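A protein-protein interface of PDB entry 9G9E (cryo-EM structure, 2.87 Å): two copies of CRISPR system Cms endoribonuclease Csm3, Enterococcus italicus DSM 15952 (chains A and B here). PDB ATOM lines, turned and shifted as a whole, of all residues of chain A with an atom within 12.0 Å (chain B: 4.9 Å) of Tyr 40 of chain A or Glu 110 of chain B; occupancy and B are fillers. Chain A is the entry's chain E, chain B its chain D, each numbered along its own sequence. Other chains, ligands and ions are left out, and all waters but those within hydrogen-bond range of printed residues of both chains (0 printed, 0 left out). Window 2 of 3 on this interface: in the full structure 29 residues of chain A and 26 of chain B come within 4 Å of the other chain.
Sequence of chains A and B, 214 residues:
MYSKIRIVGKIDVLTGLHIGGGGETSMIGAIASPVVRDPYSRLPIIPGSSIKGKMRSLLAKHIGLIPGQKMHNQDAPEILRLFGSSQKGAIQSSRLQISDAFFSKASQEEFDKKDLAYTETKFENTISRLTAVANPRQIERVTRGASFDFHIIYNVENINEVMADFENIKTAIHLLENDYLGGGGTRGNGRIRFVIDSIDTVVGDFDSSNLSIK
Position printed for both chains: 108.
Of chain A, only Tyr 40 comes within 4 Å of Glu 110 of chain B. No residue of chain A comes within 4 Å of Ser 107 of chain B. No residue of chain A comes within 4 Å of Glu 109 of chain B. Of chain A, only Tyr 40 (3.97 Å) comes within 4 Å of Phe 111 of chain B. Leu 116 of chain B touches just these residues of chain A: Pro 39 (3.3 Å) and Tyr 40 (3.6 Å). Thr 143 of chain B touches just these residues of chain A: Pro 39 (3.8 Å) and Tyr 40 (3.9 Å). Of chain A, only Tyr 40 comes within 4 Å of Gly 145 of chain B. Of the printed residues of chain B, Pro 39 of chain A touches Leu 116 and Thr 143. Of the printed residues of chain B, Ser 41 of chain A touches Arg 144 (3.996 Å). Of the printed residues of chain B, Phe 102 of chain A touches Arg 144 (3.5 Å). Of the printed residues of chain B, Asp 38 of chain A touches Arg 144 (3.0 Å). Printed residues of chain A within 4 Å of Arg 144 of chain B: Asp 38 (3.0 Å), Ser 41 (3.996 Å) and Phe 102 (3.5 Å). Val 35 of chain A touches none of the printed residues of chain B. Ile 45 of chain A touches none of the printed residues of chain B. The nearest residue of chain B that does not touch Tyr 40 of chain A is Arg 144 of chain B (4.8 Å). The nearest printed residue of chain B that does not touch Asp 38 of chain A is Thr 143 of chain B (5.1 Å).
The guanidinium group of Arg 144 of chain B is in salt-bridge range of the side-chain carboxylate of Asp 38 of chain A, at 3.0 Å. O of Tyr 40 of chain A lies within hydrogen-bond range of NZ of Lys 114 of chain B (3.3 Å). The side-chain hydroxyl (OH) of Tyr 40 of chain A sits at hydrogen-bond distance from the side-chain carboxylate (OE1) of Glu 110 of chain B, 3.2 Å away.
O of Leu 43 of chain A lies within hydrogen-bond range of N of Asp 38 of chain A (2.9 Å). O of Phe 111 of chain B lies within hydrogen-bond range of N of Leu 116 of chain B, 3.1 Å away. OD2 of Asp 38 of chain A sits at hydrogen-bond distance from OG of Ser 41 of chain A (3.2 Å).
Pro 39 of chain A touches Leu 116 of chain B. Thr 143 of chain B touches Pro 39 of chain A. Tyr 40 of chain A touches Phe 111 of chain B. Leu 116 of chain B touches Tyr 40 of chain A (CD2 to CA, 3.6 Å). N of Tyr 40 of chain A touches CG2 of Thr 143 of chain B, at 3.9 Å. Gly 145 of chain B touches Tyr 40 of chain A (CA to CD1, 3.5 Å). Ser 41 of chain A touches Arg 144 of chain B. Arg 144 of chain B touches Phe 102 of chain A.
Of the 17 printed residues of chain A, 5 touch a printed residue of chain B. Hydrophobic or aromatic side chains of chain A within 4 Å of the printed part of chain B: Pro 39, Tyr 40 and Phe 102. Along chain A the printed residues that touch a printed residue of chain B span positions 38 to 102. Of the 13 printed residues of chain B, 7 touch a printed residue of chain A. Hydrophobic or aromatic side chains of chain B that line the printed part of chain A: Phe 111 and Leu 116. Among the printed residues, 11 pairs touch across the chains. Among the printed residues, Asp or Glu carboxylates within 4 Å of a Lys or Arg side-chain nitrogen of the other chain: Asp 38 of chain A with Arg 144 of chain B (3.0 Å).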
ATOM      1  N   VAL A  35      18.665 -14.597  32.230  1.00  0.00           N
ATOM      2  CA  VAL A  35      18.561 -13.831  30.998  1.00  0.00           C
ATOM      3  C   VAL A  35      18.327 -14.791  29.839  1.00  0.00           C
ATOM      4  O   VAL A  35      18.546 -16.002  29.939  1.00  0.00           O
ATOM      5  CB  VAL A  35      19.811 -12.964  30.743  1.00  0.00           C
ATOM      6  CG1 VAL A  35      19.946 -11.906  31.818  1.00  0.00           C
ATOM      7  CG2 VAL A  35      21.057 -13.832  30.684  1.00  0.00           C
ATOM      8  N   VAL A  36      17.866 -14.231  28.720  1.00  0.00           N
ATOM      9  CA  VAL A  36      17.658 -15.026  27.518  1.00  0.00           C
ATOM     10  C   VAL A  36      19.006 -15.472  26.972  1.00  0.00           C
ATOM     11  O   VAL A  36      19.944 -14.671  26.851  1.00  0.00           O
ATOM     12  CB  VAL A  36      16.870 -14.231  26.467  1.00  0.00           C
ATOM     13  CG1 VAL A  36      15.386 -14.278  26.768  1.00  0.00           C
ATOM     14  CG2 VAL A  36      17.360 -12.798  26.412  1.00  0.00           C
ATOM     15  N   ARG A  37      19.112 -16.755  26.646  1.00  0.00           N
ATOM     16  CA  ARG A  37      20.315 -17.314  26.055  1.00  0.00           C
ATOM     17  C   ARG A  37      19.944 -18.098  24.809  1.00  0.00           C
ATOM     18  O   ARG A  37      18.864 -18.690  24.726  1.00  0.00           O
ATOM     19  CB  ARG A  37      21.061 -18.229  27.038  1.00  0.00           C
ATOM     20  CG  ARG A  37      21.256 -17.642  28.425  1.00  0.00           C
ATOM     21  CD  ARG A  37      22.053 -18.587  29.307  1.00  0.00           C
ATOM     22  NE  ARG A  37      23.489 -18.370  29.184  1.00  0.00           N
ATOM     23  CZ  ARG A  37      24.200 -17.590  29.987  1.00  0.00           C
ATOM     24  NH1 ARG A  37      23.637 -16.929  30.984  1.00  0.00           N
ATOM     25  NH2 ARG A  37      25.509 -17.469  29.782  1.00  0.00           N
ATOM     26  N   ASP A  38      20.844 -18.094  23.841  1.00  0.00           N
ATOM     27  CA  ASP A  38      20.675 -18.940  22.671  1.00  0.00           C
ATOM     28  C   ASP A  38      20.862 -20.389  23.096  1.00  0.00           C
ATOM     29  O   ASP A  38      21.909 -20.724  23.661  1.00  0.00           O
ATOM     30  CB  ASP A  38      21.678 -18.559  21.587  1.00  0.00           C
ATOM     31  CG  ASP A  38      21.528 -19.397  20.334  1.00  0.00           C
ATOM     32  OD1 ASP A  38      20.379 -19.600  19.888  1.00  0.00           O
ATOM     33  OD2 ASP A  38      22.559 -19.849  19.796  1.00  0.00           O
ATOM     34  N   PRO A  39      19.883 -21.269  22.878  1.00  0.00           N
ATOM     35  CA  PRO A  39      20.037 -22.657  23.344  1.00  0.00           C
ATOM     36  C   PRO A  39      21.231 -23.375  22.742  1.00  0.00           C
ATOM     37  O   PRO A  39      21.807 -24.253  23.396  1.00  0.00           O
ATOM     38  CB  PRO A  39      18.713 -23.312  22.926  1.00  0.00           C
ATOM     39  CG  PRO A  39      17.748 -22.178  22.816  1.00  0.00           C
ATOM     40  CD  PRO A  39      18.550 -21.022  22.304  1.00  0.00           C
ATOM     41  N   TYR A  40      21.621 -23.031  21.513  1.00  0.00           N
ATOM     42  CA  TYR A  40      22.702 -23.750  20.849  1.00  0.00           C
ATOM     43  C   TYR A  40      24.052 -23.461  21.499  1.00  0.00           C
ATOM     44  O   TYR A  40      24.822 -24.385  21.785  1.00  0.00           O
ATOM     45  CB  TYR A  40      22.729 -23.394  19.364  1.00  0.00           C
ATOM     46  CG  TYR A  40      23.624 -24.288  18.539  1.00  0.00           C
ATOM     47  CD1 TYR A  40      23.394 -25.656  18.468  1.00  0.00           C
ATOM     48  CD2 TYR A  40      24.694 -23.767  17.827  1.00  0.00           C
ATOM     49  CE1 TYR A  40      24.207 -26.479  17.714  1.00  0.00           C
ATOM     50  CE2 TYR A  40      25.514 -24.582  17.070  1.00  0.00           C
ATOM     51  CZ  TYR A  40      25.265 -25.936  17.018  1.00  0.00           C
ATOM     52  OH  TYR A  40      26.078 -26.752  16.264  1.00  0.00           O
ATOM     53  N   SER A  41      24.357 -22.187  21.739  1.00  0.00           N
ATOM     54  CA  SER A  41      25.660 -21.790  22.255  1.00  0.00           C
ATOM     55  C   SER A  41      25.653 -21.461  23.743  1.00  0.00           C
ATOM     56  O   SER A  41      26.729 -21.281  24.322  1.00  0.00           O
ATOM     57  CB  SER A  41      26.193 -20.583  21.475  1.00  0.00           C
ATOM     58  OG  SER A  41      25.260 -19.518  21.483  1.00  0.00           O
ATOM     59  N   ARG A  42      24.477 -21.375  24.365  1.00  0.00           N
ATOM     60  CA  ARG A  42      24.337 -21.012  25.777  1.00  0.00           C
ATOM     61  C   ARG A  42      24.988 -19.667  26.087  1.00  0.00           C
ATOM     62  O   ARG A  42      25.540 -19.467  27.171  1.00  0.00           O
ATOM     63  CB  ARG A  42      24.892 -22.103  26.696  1.00  0.00           C
ATOM     64  CG  ARG A  42      24.109 -23.404  26.650  1.00  0.00           C
ATOM     65  CD  ARG A  42      24.766 -24.477  27.500  1.00  0.00           C
ATOM     66  NE  ARG A  42      24.827 -24.091  28.905  1.00  0.00           N
ATOM     67  CZ  ARG A  42      23.945 -24.461  29.822  1.00  0.00           C
ATOM     68  NH1 ARG A  42      22.912 -25.231  29.518  1.00  0.00           N
ATOM     69  NH2 ARG A  42      24.100 -24.047  31.077  1.00  0.00           N
ATOM     70  N   LEU A  43      24.931 -18.730  25.129  1.00  0.00           N
ATOM     71  CA  LEU A  43      25.422 -17.375  25.300  1.00  0.00           C
ATOM     72  C   LEU A  43      24.257 -16.400  25.412  1.00  0.00           C
ATOM     73  O   LEU A  43      23.206 -16.610  24.799  1.00  0.00           O
ATOM     74  CB  LEU A  43      26.311 -16.965  24.122  1.00  0.00           C
ATOM     75  CG  LEU A  43      27.561 -17.806  23.857  1.00  0.00           C
ATOM     76  CD1 LEU A  43      28.514 -17.065  22.935  1.00  0.00           C
ATOM     77  CD2 LEU A  43      28.250 -18.175  25.158  1.00  0.00           C
ATOM     78  N   PRO A  44      24.408 -15.327  26.188  1.00  0.00           N
ATOM     79  CA  PRO A  44      23.326 -14.342  26.295  1.00  0.00           C
ATOM     80  C   PRO A  44      23.013 -13.717  24.944  1.00  0.00           C
ATOM     81  O   PRO A  44      23.891 -13.535  24.098  1.00  0.00           O
ATOM     82  CB  PRO A  44      23.879 -13.304  27.281  1.00  0.00           C
ATOM     83  CG  PRO A  44      25.352 -13.542  27.320  1.00  0.00           C
ATOM     84  CD  PRO A  44      25.541 -15.001  27.069  1.00  0.00           C
ATOM     85  N   ILE A  45      21.736 -13.392  24.747  1.00  0.00           N
ATOM     86  CA  ILE A  45      21.236 -12.916  23.467  1.00  0.00           C
ATOM     87  C   ILE A  45      20.366 -11.688  23.699  1.00  0.00           C
ATOM     88  O   ILE A  45      19.824 -11.473  24.785  1.00  0.00           O
ATOM     89  CB  ILE A  45      20.444 -14.014  22.718  1.00  0.00           C
ATOM     90  CG1 ILE A  45      20.341 -13.699  21.225  1.00  0.00           C
ATOM     91  CG2 ILE A  45      19.060 -14.193  23.328  1.00  0.00           C
ATOM     92  CD1 ILE A  45      19.394 -14.608  20.483  1.00  0.00           C
ATOM     93  N   ASP A 100      17.775 -11.026  15.860  1.00  0.00           N
ATOM     94  CA  ASP A 100      18.371 -11.286  17.162  1.00  0.00           C
ATOM     95  C   ASP A 100      19.846 -10.908  17.149  1.00  0.00           C
ATOM     96  O   ASP A 100      20.587 -11.274  16.232  1.00  0.00           O
ATOM     97  CB  ASP A 100      18.212 -12.760  17.536  1.00  0.00           C
ATOM     98  CG  ASP A 100      16.765 -13.160  17.751  1.00  0.00           C
ATOM     99  OD1 ASP A 100      15.872 -12.300  17.603  1.00  0.00           O
ATOM    100  OD2 ASP A 100      16.520 -14.341  18.070  1.00  0.00           O
ATOM    101  N   PHE A 102      23.312 -11.561  18.498  1.00  0.00           N
ATOM    102  CA  PHE A 102      24.019 -12.662  19.131  1.00  0.00           C
ATOM    103  C   PHE A 102      25.325 -12.177  19.745  1.00  0.00           C
ATOM    104  O   PHE A 102      25.940 -11.219  19.268  1.00  0.00           O
ATOM    105  CB  PHE A 102      24.301 -13.772  18.119  1.00  0.00           C
ATOM    106  CG  PHE A 102      23.066 -14.328  17.470  1.00  0.00           C
ATOM    107  CD1 PHE A 102      22.214 -15.163  18.173  1.00  0.00           C
ATOM    108  CD2 PHE A 102      22.757 -14.014  16.158  1.00  0.00           C
ATOM    109  CE1 PHE A 102      21.077 -15.674  17.577  1.00  0.00           C
ATOM    110  CE2 PHE A 102      21.622 -14.522  15.558  1.00  0.00           C
ATOM    111  CZ  PHE A 102      20.781 -15.353  16.269  1.00  0.00           C
ATOM    112  N   PHE A 103      25.734 -12.843  20.822  1.00  0.00           N
ATOM    113  CA  PHE A 103      27.007 -12.544  21.466  1.00  0.00           C
ATOM    114  C   PHE A 103      28.147 -12.658  20.464  1.00  0.00           C
ATOM    115  O   PHE A 103      28.398 -13.735  19.915  1.00  0.00           O
ATOM    116  CB  PHE A 103      27.227 -13.497  22.642  1.00  0.00           C
ATOM    117  CG  PHE A 103      28.077 -12.925  23.738  1.00  0.00           C
ATOM    118  CD1 PHE A 103      29.459 -12.978  23.662  1.00  0.00           C
ATOM    119  CD2 PHE A 103      27.494 -12.337  24.845  1.00  0.00           C
ATOM    120  CE1 PHE A 103      30.240 -12.453  24.673  1.00  0.00           C
ATOM    121  CE2 PHE A 103      28.269 -11.813  25.858  1.00  0.00           C
ATOM    122  CZ  PHE A 103      29.645 -11.870  25.771  1.00  0.00           C
ATOM    123  N   LYS A 105      31.740 -12.858  18.529  1.00  0.00           N
ATOM    124  CA  LYS A 105      32.896 -13.715  18.755  1.00  0.00           C
ATOM    125  C   LYS A 105      34.086 -12.917  19.270  1.00  0.00           C
ATOM    126  O   LYS A 105      34.907 -13.449  20.024  1.00  0.00           O
ATOM    127  CB  LYS A 105      33.259 -14.453  17.466  1.00  0.00           C
ATOM    128  CG  LYS A 105      34.289 -15.564  17.628  1.00  0.00           C
ATOM    129  CD  LYS A 105      34.084 -16.344  18.920  1.00  0.00           C
ATOM    130  CE  LYS A 105      34.987 -17.565  18.978  1.00  0.00           C
ATOM    131  NZ  LYS A 105      36.159 -17.353  19.870  1.00  0.00           N
ATOM    132  N   GLN A 108      33.535 -12.639  22.849  1.00  0.00           N
ATOM    133  CA  GLN A 108      33.805 -13.942  23.449  1.00  0.00           C
ATOM    134  C   GLN A 108      35.301 -14.167  23.634  1.00  0.00           C
ATOM    135  O   GLN A 108      35.737 -14.663  24.678  1.00  0.00           O
ATOM    136  CB  GLN A 108      33.195 -15.048  22.588  1.00  0.00           C
ATOM    137  CG  GLN A 108      33.203 -16.417  23.238  1.00  0.00           C
ATOM    138  CD  GLN A 108      32.373 -17.427  22.472  1.00  0.00           C
ATOM    139  OE1 GLN A 108      31.652 -17.074  21.539  1.00  0.00           O
ATOM    140  NE2 GLN A 108      32.473 -18.692  22.861  1.00  0.00           N
ATOM    141  N   TYR A 118      30.731 -14.235  30.783  1.00  0.00           N
ATOM    142  CA  TYR A 118      29.746 -13.698  29.844  1.00  0.00           C
ATOM    143  C   TYR A 118      28.544 -13.114  30.575  1.00  0.00           C
ATOM    144  O   TYR A 118      27.658 -12.524  29.949  1.00  0.00           O
ATOM    145  CB  TYR A 118      29.254 -14.761  28.854  1.00  0.00           C
ATOM    146  CG  TYR A 118      30.331 -15.545  28.146  1.00  0.00           C
ATOM    147  CD1 TYR A 118      31.511 -14.941  27.733  1.00  0.00           C
ATOM    148  CD2 TYR A 118      30.161 -16.896  27.885  1.00  0.00           C
ATOM    149  CE1 TYR A 118      32.490 -15.667  27.082  1.00  0.00           C
ATOM    150  CE2 TYR A 118      31.130 -17.627  27.238  1.00  0.00           C
ATOM    151  CZ  TYR A 118      32.293 -17.011  26.838  1.00  0.00           C
ATOM    152  OH  TYR A 118      33.254 -17.750  26.192  1.00  0.00           O
ATOM    153  N   ALA B 106      22.410 -35.193  10.314  1.00  0.00           N
ATOM    154  CA  ALA B 106      23.609 -34.673  10.966  1.00  0.00           C
ATOM    155  C   ALA B 106      23.245 -33.682  12.063  1.00  0.00           C
ATOM    156  O   ALA B 106      23.815 -33.719  13.161  1.00  0.00           O
ATOM    157  CB  ALA B 106      24.529 -34.023   9.934  1.00  0.00           C
ATOM    158  N   SER B 107      22.292 -32.788  11.785  1.00  0.00           N
ATOM    159  CA  SER B 107      21.796 -31.890  12.821  1.00  0.00           C
ATOM    160  C   SER B 107      21.120 -32.672  13.939  1.00  0.00           C
ATOM    161  O   SER B 107      21.201 -32.289  15.111  1.00  0.00           O
ATOM    162  CB  SER B 107      20.832 -30.871  12.215  1.00  0.00           C
ATOM    163  OG  SER B 107      20.020 -30.283  13.215  1.00  0.00           O
ATOM    164  N   GLN B 108      20.451 -33.775  13.594  1.00  0.00           N
ATOM    165  CA  GLN B 108      19.834 -34.621  14.610  1.00  0.00           C
ATOM    166  C   GLN B 108      20.878 -35.186  15.564  1.00  0.00           C
ATOM    167  O   GLN B 108      20.697 -35.152  16.785  1.00  0.00           O
ATOM    168  CB  GLN B 108      19.060 -35.756  13.942  1.00  0.00           C
ATOM    169  CG  GLN B 108      17.560 -35.704  14.136  1.00  0.00           C
ATOM    170  CD  GLN B 108      16.880 -36.960  13.634  1.00  0.00           C
ATOM    171  OE1 GLN B 108      16.301 -36.975  12.550  1.00  0.00           O
ATOM    172  NE2 GLN B 108      16.948 -38.025  14.423  1.00  0.00           N
ATOM    173  N   GLU B 109      21.979 -35.711  15.022  1.00  0.00           N
ATOM    174  CA  GLU B 109      23.043 -36.245  15.866  1.00  0.00           C
ATOM    175  C   GLU B 109      23.706 -35.143  16.684  1.00  0.00           C
ATOM    176  O   GLU B 109      24.015 -35.335  17.868  1.00  0.00           O
ATOM    177  CB  GLU B 109      24.079 -36.972  15.009  1.00  0.00           C
ATOM    178  CG  GLU B 109      23.564 -38.248  14.364  1.00  0.00           C
ATOM    179  CD  GLU B 109      24.271 -38.567  13.061  1.00  0.00           C
ATOM    180  OE1 GLU B 109      25.352 -37.993  12.814  1.00  0.00           O
ATOM    181  OE2 GLU B 109      23.744 -39.389  12.284  1.00  0.00           O
ATOM    182  N   GLU B 110      23.932 -33.980  16.069  1.00  0.00           N
ATOM    183  CA  GLU B 110      24.557 -32.874  16.784  1.00  0.00           C
ATOM    184  C   GLU B 110      23.684 -32.380  17.931  1.00  0.00           C
ATOM    185  O   GLU B 110      24.206 -31.996  18.982  1.00  0.00           O
ATOM    186  CB  GLU B 110      24.866 -31.733  15.815  1.00  0.00           C
ATOM    187  CG  GLU B 110      25.614 -30.569  16.438  1.00  0.00           C
ATOM    188  CD  GLU B 110      26.640 -29.968  15.498  1.00  0.00           C
ATOM    189  OE1 GLU B 110      26.237 -29.417  14.453  1.00  0.00           O
ATOM    190  OE2 GLU B 110      27.848 -30.049  15.803  1.00  0.00           O
ATOM    191  N   PHE B 111      22.363 -32.373  17.746  1.00  0.00           N
ATOM    192  CA  PHE B 111      21.454 -31.966  18.810  1.00  0.00           C
ATOM    193  C   PHE B 111      21.258 -33.057  19.854  1.00  0.00           C
ATOM    194  O   PHE B 111      20.993 -32.746  21.021  1.00  0.00           O
ATOM    195  CB  PHE B 111      20.106 -31.559  18.217  1.00  0.00           C
ATOM    196  CG  PHE B 111      20.044 -30.123  17.799  1.00  0.00           C
ATOM    197  CD1 PHE B 111      20.944 -29.620  16.876  1.00  0.00           C
ATOM    198  CD2 PHE B 111      19.094 -29.274  18.333  1.00  0.00           C
ATOM    199  CE1 PHE B 111      20.893 -28.300  16.493  1.00  0.00           C
ATOM    200  CE2 PHE B 111      19.039 -27.955  17.952  1.00  0.00           C
ATOM    201  CZ  PHE B 111      19.939 -27.466  17.031  1.00  0.00           C
ATOM    202  N   ASP B 112      21.358 -34.328  19.459  1.00  0.00           N
ATOM    203  CA  ASP B 112      21.349 -35.404  20.444  1.00  0.00           C
ATOM    204  C   ASP B 112      22.569 -35.311  21.348  1.00  0.00           C
ATOM    205  O   ASP B 112      22.464 -35.497  22.565  1.00  0.00           O
ATOM    206  CB  ASP B 112      21.289 -36.759  19.742  1.00  0.00           C
ATOM    207  CG  ASP B 112      19.866 -37.220  19.490  1.00  0.00           C
ATOM    208  OD1 ASP B 112      18.947 -36.700  20.157  1.00  0.00           O
ATOM    209  OD2 ASP B 112      19.667 -38.099  18.626  1.00  0.00           O
ATOM    210  N   LYS B 113      23.731 -35.022  20.769  1.00  0.00           N
ATOM    211  CA  LYS B 113      24.850 -34.557  21.570  1.00  0.00           C
ATOM    212  C   LYS B 113      24.535 -33.169  22.121  1.00  0.00           C
ATOM    213  O   LYS B 113      23.659 -32.460  21.618  1.00  0.00           O
ATOM    214  CB  LYS B 113      26.135 -34.528  20.745  1.00  0.00           C
ATOM    215  CG  LYS B 113      26.566 -35.889  20.228  1.00  0.00           C
ATOM    216  CD  LYS B 113      27.889 -35.805  19.486  1.00  0.00           C
ATOM    217  CE  LYS B 113      28.296 -37.162  18.938  1.00  0.00           C
ATOM    218  NZ  LYS B 113      27.301 -37.690  17.964  1.00  0.00           N
ATOM    219  N   LYS B 114      25.243 -32.792  23.185  1.00  0.00           N
ATOM    220  CA  LYS B 114      25.036 -31.558  23.938  1.00  0.00           C
ATOM    221  C   LYS B 114      23.705 -31.546  24.683  1.00  0.00           C
ATOM    222  O   LYS B 114      23.408 -30.557  25.366  1.00  0.00           O
ATOM    223  CB  LYS B 114      25.112 -30.300  23.059  1.00  0.00           C
ATOM    224  CG  LYS B 114      26.307 -30.245  22.124  1.00  0.00           C
ATOM    225  CD  LYS B 114      25.924 -29.624  20.788  1.00  0.00           C
ATOM    226  CE  LYS B 114      25.354 -28.226  20.962  1.00  0.00           C
ATOM    227  NZ  LYS B 114      26.388 -27.257  21.415  1.00  0.00           N
ATOM    228  N   LEU B 116      20.657 -31.152  23.664  1.00  0.00           N
ATOM    229  CA  LEU B 116      19.910 -29.988  23.206  1.00  0.00           C
ATOM    230  C   LEU B 116      18.611 -30.427  22.544  1.00  0.00           C
ATOM    231  O   LEU B 116      18.612 -31.325  21.696  1.00  0.00           O
ATOM    232  CB  LEU B 116      20.745 -29.162  22.228  1.00  0.00           C
ATOM    233  CG  LEU B 116      20.206 -27.775  21.880  1.00  0.00           C
ATOM    234  CD1 LEU B 116      19.910 -26.983  23.142  1.00  0.00           C
ATOM    235  CD2 LEU B 116      21.191 -27.037  20.996  1.00  0.00           C
ATOM    236  N   THR B 143      15.625 -24.458  17.022  1.00  0.00           N
ATOM    237  CA  THR B 143      16.866 -23.929  17.572  1.00  0.00           C
ATOM    238  C   THR B 143      17.835 -23.541  16.458  1.00  0.00           C
ATOM    239  O   THR B 143      17.880 -24.164  15.394  1.00  0.00           O
ATOM    240  CB  THR B 143      17.503 -24.959  18.509  1.00  0.00           C
ATOM    241  OG1 THR B 143      16.539 -25.372  19.485  1.00  0.00           O
ATOM    242  CG2 THR B 143      18.708 -24.373  19.230  1.00  0.00           C
ATOM    243  N   ARG B 144      18.612 -22.486  16.719  1.00  0.00           N
ATOM    244  CA  ARG B 144      19.482 -21.885  15.713  1.00  0.00           C
ATOM    245  C   ARG B 144      20.533 -22.856  15.178  1.00  0.00           C
ATOM    246  O   ARG B 144      20.998 -22.688  14.048  1.00  0.00           O
ATOM    247  CB  ARG B 144      20.134 -20.635  16.318  1.00  0.00           C
ATOM    248  CG  ARG B 144      21.433 -20.170  15.686  1.00  0.00           C
ATOM    249  CD  ARG B 144      21.869 -18.854  16.309  1.00  0.00           C
ATOM    250  NE  ARG B 144      23.121 -18.354  15.753  1.00  0.00           N
ATOM    251  CZ  ARG B 144      24.254 -18.253  16.434  1.00  0.00           C
ATOM    252  NH1 ARG B 144      24.330 -18.613  17.704  1.00  0.00           N
ATOM    253  NH2 ARG B 144      25.335 -17.775  15.826  1.00  0.00           N
ATOM    254  N   GLY B 145      20.901 -23.880  15.939  1.00  0.00           N
ATOM    255  CA  GLY B 145      21.877 -24.818  15.417  1.00  0.00           C
ATOM    256  C   GLY B 145      21.342 -25.816  14.413  1.00  0.00           C
ATOM    257  O   GLY B 145      22.128 -26.573  13.836  1.00  0.00           O
